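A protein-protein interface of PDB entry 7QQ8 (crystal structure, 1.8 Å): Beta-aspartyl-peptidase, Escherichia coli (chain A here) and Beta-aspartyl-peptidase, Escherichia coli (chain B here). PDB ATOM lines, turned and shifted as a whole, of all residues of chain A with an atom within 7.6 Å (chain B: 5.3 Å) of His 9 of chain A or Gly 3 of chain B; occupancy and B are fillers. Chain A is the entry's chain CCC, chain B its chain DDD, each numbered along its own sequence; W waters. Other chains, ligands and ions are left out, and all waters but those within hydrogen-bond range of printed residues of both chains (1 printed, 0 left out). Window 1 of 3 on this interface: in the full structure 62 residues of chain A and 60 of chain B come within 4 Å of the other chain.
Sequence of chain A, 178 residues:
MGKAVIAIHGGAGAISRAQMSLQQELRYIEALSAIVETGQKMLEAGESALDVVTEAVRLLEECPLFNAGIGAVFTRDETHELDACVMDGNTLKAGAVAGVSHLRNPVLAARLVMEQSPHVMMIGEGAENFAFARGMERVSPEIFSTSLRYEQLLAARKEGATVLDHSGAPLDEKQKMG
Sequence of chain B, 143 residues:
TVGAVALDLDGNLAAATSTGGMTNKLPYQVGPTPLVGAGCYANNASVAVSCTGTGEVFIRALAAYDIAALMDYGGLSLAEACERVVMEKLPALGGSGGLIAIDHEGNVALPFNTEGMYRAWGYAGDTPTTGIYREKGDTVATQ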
ATOM      1  N   ILE A   6       7.933  10.660  12.466  1.00  0.00           N
ATOM      2  CA  ILE A   6       8.173   9.234  12.819  1.00  0.00           C
ATOM      3  C   ILE A   6       6.973   8.413  12.348  1.00  0.00           C
ATOM      4  O   ILE A   6       5.804   8.878  12.493  1.00  0.00           O
ATOM      5  CB  ILE A   6       8.490   9.013  14.321  1.00  0.00           C
ATOM      6  CG1 ILE A   6       8.569   7.511  14.645  1.00  0.00           C
ATOM      7  CG2 ILE A   6       7.467   9.718  15.214  1.00  0.00           C
ATOM      8  CD1 ILE A   6       9.107   7.169  16.003  1.00  0.00           C
ATOM      9  N   ALA A   7       7.245   7.197  11.883  1.00  0.00           N
ATOM     10  CA  ALA A   7       6.203   6.154  11.737  1.00  0.00           C
ATOM     11  C   ALA A   7       6.685   4.874  12.403  1.00  0.00           C
ATOM     12  O   ALA A   7       7.923   4.678  12.436  1.00  0.00           O
ATOM     13  CB  ALA A   7       5.881   5.948  10.297  1.00  0.00           C
ATOM     14  N   ILE A   8       5.763   4.097  12.968  1.00  0.00           N
ATOM     15  CA  ILE A   8       6.041   2.779  13.600  1.00  0.00           C
ATOM     16  C   ILE A   8       5.035   1.767  13.080  1.00  0.00           C
ATOM     17  O   ILE A   8       3.947   2.141  12.631  1.00  0.00           O
ATOM     18  CB  ILE A   8       6.061   2.834  15.146  1.00  0.00           C
ATOM     19  CG1 ILE A   8       4.689   3.141  15.762  1.00  0.00           C
ATOM     20  CG2 ILE A   8       7.104   3.815  15.588  1.00  0.00           C
ATOM     21  CD1 ILE A   8       4.627   3.110  17.283  1.00  0.00           C
ATOM     22  N   HIS A   9       5.399   0.514  13.173  1.00  0.00           N
ATOM     23  CA  HIS A   9       4.447  -0.597  12.994  1.00  0.00           C
ATOM     24  C   HIS A   9       4.732  -1.658  14.037  1.00  0.00           C
ATOM     25  O   HIS A   9       5.886  -1.731  14.541  1.00  0.00           O
ATOM     26  CB  HIS A   9       4.453  -1.154  11.568  1.00  0.00           C
ATOM     27  CG  HIS A   9       5.637  -2.007  11.235  1.00  0.00           C
ATOM     28  ND1 HIS A   9       5.743  -3.323  11.666  1.00  0.00           N
ATOM     29  CD2 HIS A   9       6.792  -1.707  10.610  1.00  0.00           C
ATOM     30  CE1 HIS A   9       6.878  -3.835  11.244  1.00  0.00           C
ATOM     31  NE2 HIS A   9       7.549  -2.836  10.590  1.00  0.00           N
ATOM     32  N   GLY A  10       3.712  -2.480  14.259  1.00  0.00           N
ATOM     33  CA  GLY A  10       3.771  -3.646  15.146  1.00  0.00           C
ATOM     34  C   GLY A  10       3.350  -4.899  14.435  1.00  0.00           C
ATOM     35  O   GLY A  10       2.892  -5.865  15.143  1.00  0.00           O
ATOM     36  N   GLY A  11       3.462  -4.896  13.106  1.00  0.00           N
ATOM     37  CA  GLY A  11       3.234  -6.097  12.297  1.00  0.00           C
ATOM     38  C   GLY A  11       1.919  -6.007  11.526  1.00  0.00           C
ATOM     39  O   GLY A  11       0.996  -5.239  11.935  1.00  0.00           O
ATOM     40  N   ALA A  12       1.879  -6.708  10.397  1.00  0.00           N
ATOM     41  CA  ALA A  12       0.752  -6.771   9.447  1.00  0.00           C
ATOM     42  C   ALA A  12       0.267  -8.212   9.451  1.00  0.00           C
ATOM     43  O   ALA A  12       1.124  -9.111   9.576  1.00  0.00           O
ATOM     44  CB  ALA A  12       1.186  -6.341   8.068  1.00  0.00           C
ATOM     45  N   LEU A  32       0.886   1.880  20.811  1.00  0.00           N
ATOM     46  CA  LEU A  32       1.310   2.591  19.585  1.00  0.00           C
ATOM     47  C   LEU A  32       1.397   4.107  19.851  1.00  0.00           C
ATOM     48  O   LEU A  32       2.372   4.752  19.403  1.00  0.00           O
ATOM     49  CB  LEU A  32       0.329   2.261  18.469  1.00  0.00           C
ATOM     50  CG  LEU A  32       0.370   0.842  17.913  1.00  0.00           C
ATOM     51  CD1 LEU A  32      -0.812   0.625  16.989  1.00  0.00           C
ATOM     52  CD2 LEU A  32       1.642   0.572  17.123  1.00  0.00           C
ATOM     53  N   ILE A  35       4.455   5.107  22.199  1.00  0.00           N
ATOM     54  CA  ILE A  35       5.774   4.916  21.527  1.00  0.00           C
ATOM     55  C   ILE A  35       5.913   5.992  20.457  1.00  0.00           C
ATOM     56  O   ILE A  35       6.968   6.661  20.470  1.00  0.00           O
ATOM     57  CB  ILE A  35       5.884   3.481  20.996  1.00  0.00           C
ATOM     58  CG1 ILE A  35       5.838   2.478  22.150  1.00  0.00           C
ATOM     59  CG2 ILE A  35       7.131   3.322  20.135  1.00  0.00           C
ATOM     60  CD1 ILE A  35       5.669   1.049  21.725  1.00  0.00           C
ATOM     61  N   VAL A  53      14.622   5.818  15.981  1.00  0.00           N
ATOM     62  CA  VAL A  53      14.082   4.496  15.529  1.00  0.00           C
ATOM     63  C   VAL A  53      14.620   3.405  16.469  1.00  0.00           C
ATOM     64  O   VAL A  53      13.930   2.386  16.681  1.00  0.00           O
ATOM     65  CB  VAL A  53      14.400   4.188  14.059  1.00  0.00           C
ATOM     66  CG1 VAL A  53      13.820   5.287  13.179  1.00  0.00           C
ATOM     67  CG2 VAL A  53      15.900   4.009  13.804  1.00  0.00           C
ATOM     68  N   ALA A  56      12.314   3.551  19.596  1.00  0.00           N
ATOM     69  CA  ALA A  56      10.927   3.169  19.254  1.00  0.00           C
ATOM     70  C   ALA A  56      10.903   1.638  19.133  1.00  0.00           C
ATOM     71  O   ALA A  56      10.059   1.001  19.754  1.00  0.00           O
ATOM     72  CB  ALA A  56      10.470   3.829  18.000  1.00  0.00           C
ATOM     73  N   VAL A  57      11.888   1.050  18.449  1.00  0.00           N
ATOM     74  CA  VAL A  57      11.880  -0.407  18.232  1.00  0.00           C
ATOM     75  C   VAL A  57      12.184  -1.097  19.576  1.00  0.00           C
ATOM     76  O   VAL A  57      11.594  -2.146  19.822  1.00  0.00           O
ATOM     77  CB  VAL A  57      12.831  -0.830  17.104  1.00  0.00           C
ATOM     78  CG1 VAL A  57      13.028  -2.337  17.077  1.00  0.00           C
ATOM     79  CG2 VAL A  57      12.282  -0.351  15.772  1.00  0.00           C
ATOM     80  N   LEU A  60       8.879  -1.257  21.305  1.00  0.00           N
ATOM     81  CA  LEU A  60       8.003  -2.243  20.636  1.00  0.00           C
ATOM     82  C   LEU A  60       8.447  -3.645  21.030  1.00  0.00           C
ATOM     83  O   LEU A  60       7.602  -4.569  21.129  1.00  0.00           O
ATOM     84  CB  LEU A  60       8.084  -1.987  19.134  1.00  0.00           C
ATOM     85  CG  LEU A  60       7.374  -0.713  18.670  1.00  0.00           C
ATOM     86  CD1 LEU A  60       7.807  -0.263  17.283  1.00  0.00           C
ATOM     87  CD2 LEU A  60       5.852  -0.839  18.704  1.00  0.00           C
ATOM     88  N   PHE A  66       3.509  -7.208  20.900  1.00  0.00           N
ATOM     89  CA  PHE A  66       4.106  -7.227  19.553  1.00  0.00           C
ATOM     90  C   PHE A  66       5.184  -8.312  19.489  1.00  0.00           C
ATOM     91  O   PHE A  66       5.942  -8.568  20.507  1.00  0.00           O
ATOM     92  CB  PHE A  66       4.618  -5.844  19.193  1.00  0.00           C
ATOM     93  CG  PHE A  66       3.562  -4.770  19.210  1.00  0.00           C
ATOM     94  CD1 PHE A  66       2.454  -4.855  18.399  1.00  0.00           C
ATOM     95  CD2 PHE A  66       3.708  -3.636  20.013  1.00  0.00           C
ATOM     96  CE1 PHE A  66       1.478  -3.870  18.420  1.00  0.00           C
ATOM     97  CE2 PHE A  66       2.741  -2.629  19.993  1.00  0.00           C
ATOM     98  CZ  PHE A  66       1.621  -2.753  19.199  1.00  0.00           C
ATOM     99  N   ALA A  68       8.245  -9.267  18.795  1.00  0.00           N
ATOM    100  CA  ALA A  68       9.646  -8.785  18.756  1.00  0.00           C
ATOM    101  C   ALA A  68      10.020  -8.680  20.218  1.00  0.00           C
ATOM    102  O   ALA A  68       9.117  -8.295  20.989  1.00  0.00           O
ATOM    103  CB  ALA A  68       9.795  -7.492  17.997  1.00  0.00           C
ATOM    104  N   CYS A  85      17.397  -5.369  12.551  1.00  0.00           N
ATOM    105  CA  CYS A  85      18.256  -4.581  11.653  1.00  0.00           C
ATOM    106  C   CYS A  85      18.061  -3.109  11.989  1.00  0.00           C
ATOM    107  O   CYS A  85      16.994  -2.757  12.464  1.00  0.00           O
ATOM    108  CB  CYS A  85      17.943  -4.857  10.183  1.00  0.00           C
ATOM    109  SG  CYS A  85      19.151  -4.099   9.067  1.00  0.00           S
ATOM    110  N   THR B   1       6.731  -8.964  14.194  1.00  0.00           N
ATOM    111  CA  THR B   1       7.639  -7.991  13.558  1.00  0.00           C
ATOM    112  C   THR B   1       7.173  -6.600  13.996  1.00  0.00           C
ATOM    113  O   THR B   1       5.954  -6.360  14.128  1.00  0.00           O
ATOM    114  CB  THR B   1       7.710  -8.157  12.034  1.00  0.00           C
ATOM    115  OG1 THR B   1       8.056  -9.517  11.786  1.00  0.00           O
ATOM    116  CG2 THR B   1       8.776  -7.288  11.386  1.00  0.00           C
ATOM    117  N   VAL B   2       8.140  -5.727  14.238  1.00  0.00           N
ATOM    118  CA  VAL B   2       7.905  -4.324  14.605  1.00  0.00           C
ATOM    119  C   VAL B   2       8.917  -3.477  13.856  1.00  0.00           C
ATOM    120  O   VAL B   2       9.989  -4.011  13.453  1.00  0.00           O
ATOM    121  CB  VAL B   2       8.034  -4.118  16.124  1.00  0.00           C
ATOM    122  CG1 VAL B   2       7.053  -5.008  16.872  1.00  0.00           C
ATOM    123  CG2 VAL B   2       9.466  -4.271  16.644  1.00  0.00           C
ATOM    124  N   GLY B   3       8.648  -2.189  13.754  1.00  0.00           N
ATOM    125  CA  GLY B   3       9.625  -1.303  13.105  1.00  0.00           C
ATOM    126  C   GLY B   3       9.327   0.173  13.300  1.00  0.00           C
ATOM    127  O   GLY B   3       8.246   0.549  13.783  1.00  0.00           O
ATOM    128  N   ALA B   4      10.313   0.987  12.948  1.00  0.00           N
ATOM    129  CA  ALA B   4      10.270   2.459  13.042  1.00  0.00           C
ATOM    130  C   ALA B   4      11.067   3.035  11.883  1.00  0.00           C
ATOM    131  O   ALA B   4      12.128   2.495  11.514  1.00  0.00           O
ATOM    132  CB  ALA B   4      10.813   2.935  14.362  1.00  0.00           C
ATOM    133  N   VAL B   5      10.595   4.157  11.391  1.00  0.00           N
ATOM    134  CA  VAL B   5      11.326   5.009  10.436  1.00  0.00           C
ATOM    135  C   VAL B   5      11.173   6.450  10.915  1.00  0.00           C
ATOM    136  O   VAL B   5      10.185   6.782  11.544  1.00  0.00           O
ATOM    137  CB  VAL B   5      10.800   4.860   9.003  1.00  0.00           C
ATOM    138  CG1 VAL B   5      11.164   3.499   8.447  1.00  0.00           C
ATOM    139  CG2 VAL B   5       9.294   5.099   8.918  1.00  0.00           C
ATOM    140  N   ALA B  16      14.573   0.874  11.448  1.00  0.00           N
ATOM    141  CA  ALA B  16      14.873  -0.265  12.304  1.00  0.00           C
ATOM    142  C   ALA B  16      13.710  -1.234  12.303  1.00  0.00           C
ATOM    143  O   ALA B  16      12.564  -0.815  12.115  1.00  0.00           O
ATOM    144  CB  ALA B  16      15.220   0.269  13.675  1.00  0.00           C
ATOM    145  N   THR B  17      14.014  -2.522  12.428  1.00  0.00           N
ATOM    146  CA  THR B  17      13.025  -3.615  12.351  1.00  0.00           C
ATOM    147  C   THR B  17      13.486  -4.698  13.311  1.00  0.00           C
ATOM    148  O   THR B  17      14.711  -4.878  13.441  1.00  0.00           O
ATOM    149  CB  THR B  17      12.925  -4.187  10.937  1.00  0.00           C
ATOM    150  OG1 THR B  17      12.777  -3.084  10.043  1.00  0.00           O
ATOM    151  CG2 THR B  17      11.806  -5.178  10.786  1.00  0.00           C
ATOM    152  N   SER B  18      12.554  -5.373  13.964  1.00  0.00           N
ATOM    153  CA  SER B  18      12.889  -6.408  14.969  1.00  0.00           C
ATOM    154  C   SER B  18      11.770  -7.435  14.896  1.00  0.00           C
ATOM    155  O   SER B  18      10.638  -7.035  14.661  1.00  0.00           O
ATOM    156  CB  SER B  18      13.106  -5.785  16.357  1.00  0.00           C
ATOM    157  OG  SER B  18      13.510  -6.767  17.306  1.00  0.00           O
ATOM    158  N   SER B  50      10.731   0.224   6.782  1.00  0.00           N
ATOM    159  CA  SER B  50      10.664  -0.943   7.682  1.00  0.00           C
ATOM    160  C   SER B  50       9.491  -1.789   7.219  1.00  0.00           C
ATOM    161  O   SER B  50       8.396  -1.237   7.095  1.00  0.00           O
ATOM    162  CB  SER B  50      10.549  -0.587   9.144  1.00  0.00           C
ATOM    163  OG  SER B  50      10.426  -1.802   9.877  1.00  0.00           O
ATOM    164  N   CYS B  51       9.740  -3.057   6.926  1.00  0.00           N
ATOM    165  CA  CYS B  51       8.733  -3.983   6.380  1.00  0.00           C
ATOM    166  C   CYS B  51       8.203  -4.933   7.447  1.00  0.00           C
ATOM    167  O   CYS B  51       8.917  -5.232   8.391  1.00  0.00           O
ATOM    168  CB  CYS B  51       9.331  -4.781   5.226  1.00  0.00           C
ATOM    169  SG  CYS B  51       9.777  -3.731   3.815  1.00  0.00           S
ATOM    170  N   THR B  52       6.996  -5.429   7.241  1.00  0.00           N
ATOM    171  CA  THR B  52       6.439  -6.596   7.951  1.00  0.00           C
ATOM    172  C   THR B  52       5.573  -7.437   7.017  1.00  0.00           C
ATOM    173  O   THR B  52       4.614  -6.863   6.498  1.00  0.00           O
ATOM    174  CB  THR B  52       5.525  -6.118   9.071  1.00  0.00           C
ATOM    175  OG1 THR B  52       4.734  -7.236   9.463  1.00  0.00           O
ATOM    176  CG2 THR B  52       4.594  -4.977   8.723  1.00  0.00           C
ATOM    177  N   ILE B 100       6.257   0.654   6.362  1.00  0.00           N
ATOM    178  CA  ILE B 100       6.205   2.088   6.732  1.00  0.00           C
ATOM    179  C   ILE B 100       7.406   2.737   6.060  1.00  0.00           C
ATOM    180  O   ILE B 100       8.425   2.074   5.888  1.00  0.00           O
ATOM    181  CB  ILE B 100       6.145   2.277   8.268  1.00  0.00           C
ATOM    182  CG1 ILE B 100       7.391   1.722   8.967  1.00  0.00           C
ATOM    183  CG2 ILE B 100       4.884   1.640   8.797  1.00  0.00           C
ATOM    184  CD1 ILE B 100       7.427   1.952  10.450  1.00  0.00           C
ATOM    185  N   MET B 117      -2.689  -3.675   9.978  1.00  0.00           N
ATOM    186  CA  MET B 117      -1.277  -3.463  10.339  1.00  0.00           C
ATOM    187  C   MET B 117      -1.276  -2.535  11.535  1.00  0.00           C
ATOM    188  O   MET B 117      -1.796  -1.456  11.432  1.00  0.00           O
ATOM    189  CB  MET B 117      -0.451  -2.870   9.198  1.00  0.00           C
ATOM    190  CG  MET B 117       0.981  -2.615   9.573  1.00  0.00           C
ATOM    191  SD  MET B 117       2.040  -2.287   8.167  1.00  0.00           S
ATOM    192  CE  MET B 117       1.709  -0.557   7.832  1.00  0.00           C
ATOM    193  N   TYR B 118      -0.758  -3.005  12.655  1.00  0.00           N
ATOM    194  CA  TYR B 118      -0.597  -2.156  13.855  1.00  0.00           C
ATOM    195  C   TYR B 118       0.368  -1.045  13.488  1.00  0.00           C
ATOM    196  O   TYR B 118       1.461  -1.383  13.094  1.00  0.00           O
ATOM    197  CB  TYR B 118      -0.100  -2.989  15.023  1.00  0.00           C
ATOM    198  CG  TYR B 118      -1.027  -4.088  15.472  1.00  0.00           C
ATOM    199  CD1 TYR B 118      -2.275  -3.818  16.012  1.00  0.00           C
ATOM    200  CD2 TYR B 118      -0.598  -5.409  15.450  1.00  0.00           C
ATOM    201  CE1 TYR B 118      -3.095  -4.840  16.457  1.00  0.00           C
ATOM    202  CE2 TYR B 118      -1.405  -6.443  15.890  1.00  0.00           C
ATOM    203  CZ  TYR B 118      -2.666  -6.153  16.392  1.00  0.00           C
ATOM    204  OH  TYR B 118      -3.427  -7.187  16.861  1.00  0.00           O
ATOM    205  N   ARG B 119      -0.042   0.209  13.542  1.00  0.00           N
ATOM    206  CA  ARG B 119       0.770   1.320  12.982  1.00  0.00           C
ATOM    207  C   ARG B 119       0.487   2.658  13.648  1.00  0.00           C
ATOM    208  O   ARG B 119      -0.613   2.843  14.229  1.00  0.00           O
ATOM    209  CB  ARG B 119       0.509   1.467  11.498  1.00  0.00           C
ATOM    210  CG  ARG B 119      -0.925   1.819  11.179  1.00  0.00           C
ATOM    211  CD  ARG B 119      -1.148   1.550   9.724  1.00  0.00           C
ATOM    212  NE  ARG B 119      -2.425   2.148   9.299  1.00  0.00           N
ATOM    213  CZ  ARG B 119      -3.600   1.534   9.468  1.00  0.00           C
ATOM    214  NH1 ARG B 119      -3.679   0.355  10.079  1.00  0.00           N
ATOM    215  NH2 ARG B 119      -4.698   2.107   9.037  1.00  0.00           N
ATOM    216  N   ALA B 120       1.428   3.581  13.521  1.00  0.00           N
ATOM    217  CA  ALA B 120       1.236   4.948  14.037  1.00  0.00           C
ATOM    218  C   ALA B 120       2.240   5.870  13.388  1.00  0.00           C
ATOM    219  O   ALA B 120       3.292   5.405  12.943  1.00  0.00           O
ATOM    220  CB  ALA B 120       1.332   4.989  15.556  1.00  0.00           C
HETATM  221  O   HOH W   1       3.881  -8.095  15.981  1.00  0.00           O
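Of the printed residues of chain B, Ile 6 of chain A touches Val 5. Of chain B, only Thr 1 (3.9 Å), Val 2 (3.3 Å), Gly 3 (2.9 Å), Ser 50 (3.1 Å), Cys 51 (3.5 Å), Thr 52 (3.4 Å), Ile 100 (3.7 Å) and Tyr 118 (3.1 Å) come within 4 Å of His 9 of chain A. Of the printed residues of chain B, Leu 32 of chain A touches Arg 119 (3.5 Å) and Ala 120 (3.99 Å). Printed residues of chain B within 4 Å of Val 53 of chain A: Ala 4 (3.7 Å), Val 5 (3.7 Å) and Ala 16 (3.8 Å). Printed residues of chain B within 4 Å of Cys 85 of chain A: Ala 16 and Thr 17. Printed residues of chain A within 4 Å of Gly 3 of chain B: Ile 8 (3.1 Å), His 9 (2.9 Å), Val 57 (3.9 Å) and Leu 60 (3.6 Å). Of the printed residues of chain A, Cys 51 of chain B touches His 9 (3.5 Å). The nearest residue of chain B that does not touch His 9 of chain A is Arg 119 of chain B (4.1 Å). The nearest residue of chain A that does not touch Gly 3 of chain B is Ala 7 of chain A (4.4 Å).
The backbone NH (N) of Ala 16 of chain B is in hydrogen-bond range of the backbone carbonyl oxygen (O) of Ala 4 of chain B, 2.9 Å away. OG of Ser 50 of chain B sits at hydrogen-bond distance from OG1 of Thr 17 of chain B (2.7 Å). O of Ser 50 of chain B sits at hydrogen-bond distance from N of Ile 100 of chain B. A ring nitrogen (ND1) of His 9 of chain A sits at hydrogen-bond distance from the backbone NH of Gly 11 of chain A (3.1 Å). NH1 of Arg 119 of chain B sits at hydrogen-bond distance from O of Met 117 of chain B. The backbone carbonyl oxygen (O) of Ala 16 of chain B sits at hydrogen-bond distance from the side-chain hydroxyl (OG) of Ser 50 of chain B (3.2 Å).
Water W1 bridges the backbone carbonyl oxygen (O) of Gly 10 of chain A (2.6 Å) and the backbone carbonyl oxygen (O) of Thr 1 of chain B (3.3 Å).
Among the printed residues, merely in contact across the chains: His 9 of chain A with Tyr 118 of chain B (3.1 Å), Ile 8 of chain A with Gly 3 of chain B (3.1 Å), Ala 7 of chain A with Ala 120 of chain B (3.2 Å), Cys 85 of chain A with Ala 16 of chain B (3.3 Å), Ala 7 of chain A with Ala 4 of chain B (3.3 Å), His 9 of chain A with Val 2 of chain B (3.3 Å), Gly 11 of chain A with Met 117 of chain B (3.3 Å), Ile 8 of chain A with Arg 119 of chain B (3.3 Å), Gly 11 of chain A with Thr 52 of chain B (3.4 Å), Ala 7 of chain A with Ile 100 of chain B (3.4 Å), Ile 6 of chain A with Val 5 of chain B (3.4 Å), His 9 of chain A with Thr 52 of chain B (3.4 Å), Phe 66 of chain A with Val 2 of chain B (3.5 Å), Ala 68 of chain A with Ser 18 of chain B (3.5 Å), Ala 68 of chain A with Val 2 of chain B (3.5 Å), Val 57 of chain A with Ser 18 of chain B (3.5 Å), His 9 of chain A with Cys 51 of chain B (3.5 Å), Ile 8 of chain A with Ile 100 of chain B (3.5 Å), Leu 32 of chain A with Arg 119 of chain B (3.5 Å), Leu 60 of chain A with Gly 3 of chain B (3.6 Å), Leu 60 of chain A with Val 2 of chain B (3.7 Å), Val 57 of chain A with Ala 16 of chain B (3.7 Å), Val 53 of chain A with Ala 4 of chain B (3.7 Å), Val 53 of chain A with Val 5 of chain B (3.7 Å), His 9 of chain A with Ile 100 of chain B (3.7 Å), Val 57 of chain A with Ala 4 of chain B (3.7 Å), Ala 56 of chain A with Ala 4 of chain B (3.8 Å), Val 53 of chain A with Ala 16 of chain B (3.8 Å), Phe 66 of chain A with Tyr 118 of chain B (3.8 Å), Val 57 of chain A with Gly 3 of chain B (3.9 Å), His 9 of chain A with Thr 1 of chain B (3.9 Å), Gly 10 of chain A with Val 2 of chain B (3.95 Å), Ala 12 of chain A with Met 117 of chain B (3.98 Å) and Leu 32 of chain A with Ala 120 of chain B (3.99 Å).
Printed residues of chain B that touch a printed residue of chain A: Thr 1, Val 2, Gly 3, Ala 4, Val 5, Ala 16, Thr 17, Ser 18, Ser 50, Cys 51, Thr 52, Ile 100, Met 117, Tyr 118, Arg 119 and Ala 120. Hydrophobic or aromatic side chains of chain B that line the printed part of chain A: Val 2, Ala 4, Val 5, Ala 16, Ile 100, Met 117, Tyr 118 and Ala 120. Along chain B the printed residues that touch a printed residue of chain A span positions 1 to 120. Of the 16 printed residues of chain A, 15 touch a printed residue of chain B. Among the printed residues, no Asp or Glu carboxylate lies within 4 Å of a Lys or Arg side-chain nitrogen of the other chain.
O of Gly 10 of chain A sits close to O of Thr 1 of chain B. OG1 of Thr 52 of chain B lies within hydrogen-bond range of N of Ala 12 of chain A (3.0 Å). N of Tyr 118 of chain B sits at hydrogen-bond distance from O of Gly 11 of chain A (2.9 Å). N of Gly 3 of chain B lies within hydrogen-bond range of O of His 9 of chain A. A ring nitrogen (NE2) of His 9 of chain A lies within hydrogen-bond range of the side-chain hydroxyl (OG) of Ser 50 of chain B (3.1 Å). The backbone NH (N) of Cys 85 of chain A sits at hydrogen-bond distance from the backbone carbonyl oxygen (O) of Thr 17 of chain B (2.9 Å). The backbone NH (N) of Ile 8 of chain A sits at hydrogen-bond distance from the backbone carbonyl oxygen (O) of Ala 120 of chain B, 2.8 Å away. The backbone NH (N) of Gly 10 of chain A sits at hydrogen-bond distance from the backbone carbonyl oxygen (O) of Tyr 118 of chain B (2.8 Å). The backbone NH (N) of Gly 11 of chain A is in hydrogen-bond range of the backbone carbonyl oxygen (O) of Thr 1 of chain B. The backbone carbonyl oxygen of Ala 7 of chain A lies within hydrogen-bond range of the backbone NH of Val 5 of chain B (2.9 Å).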
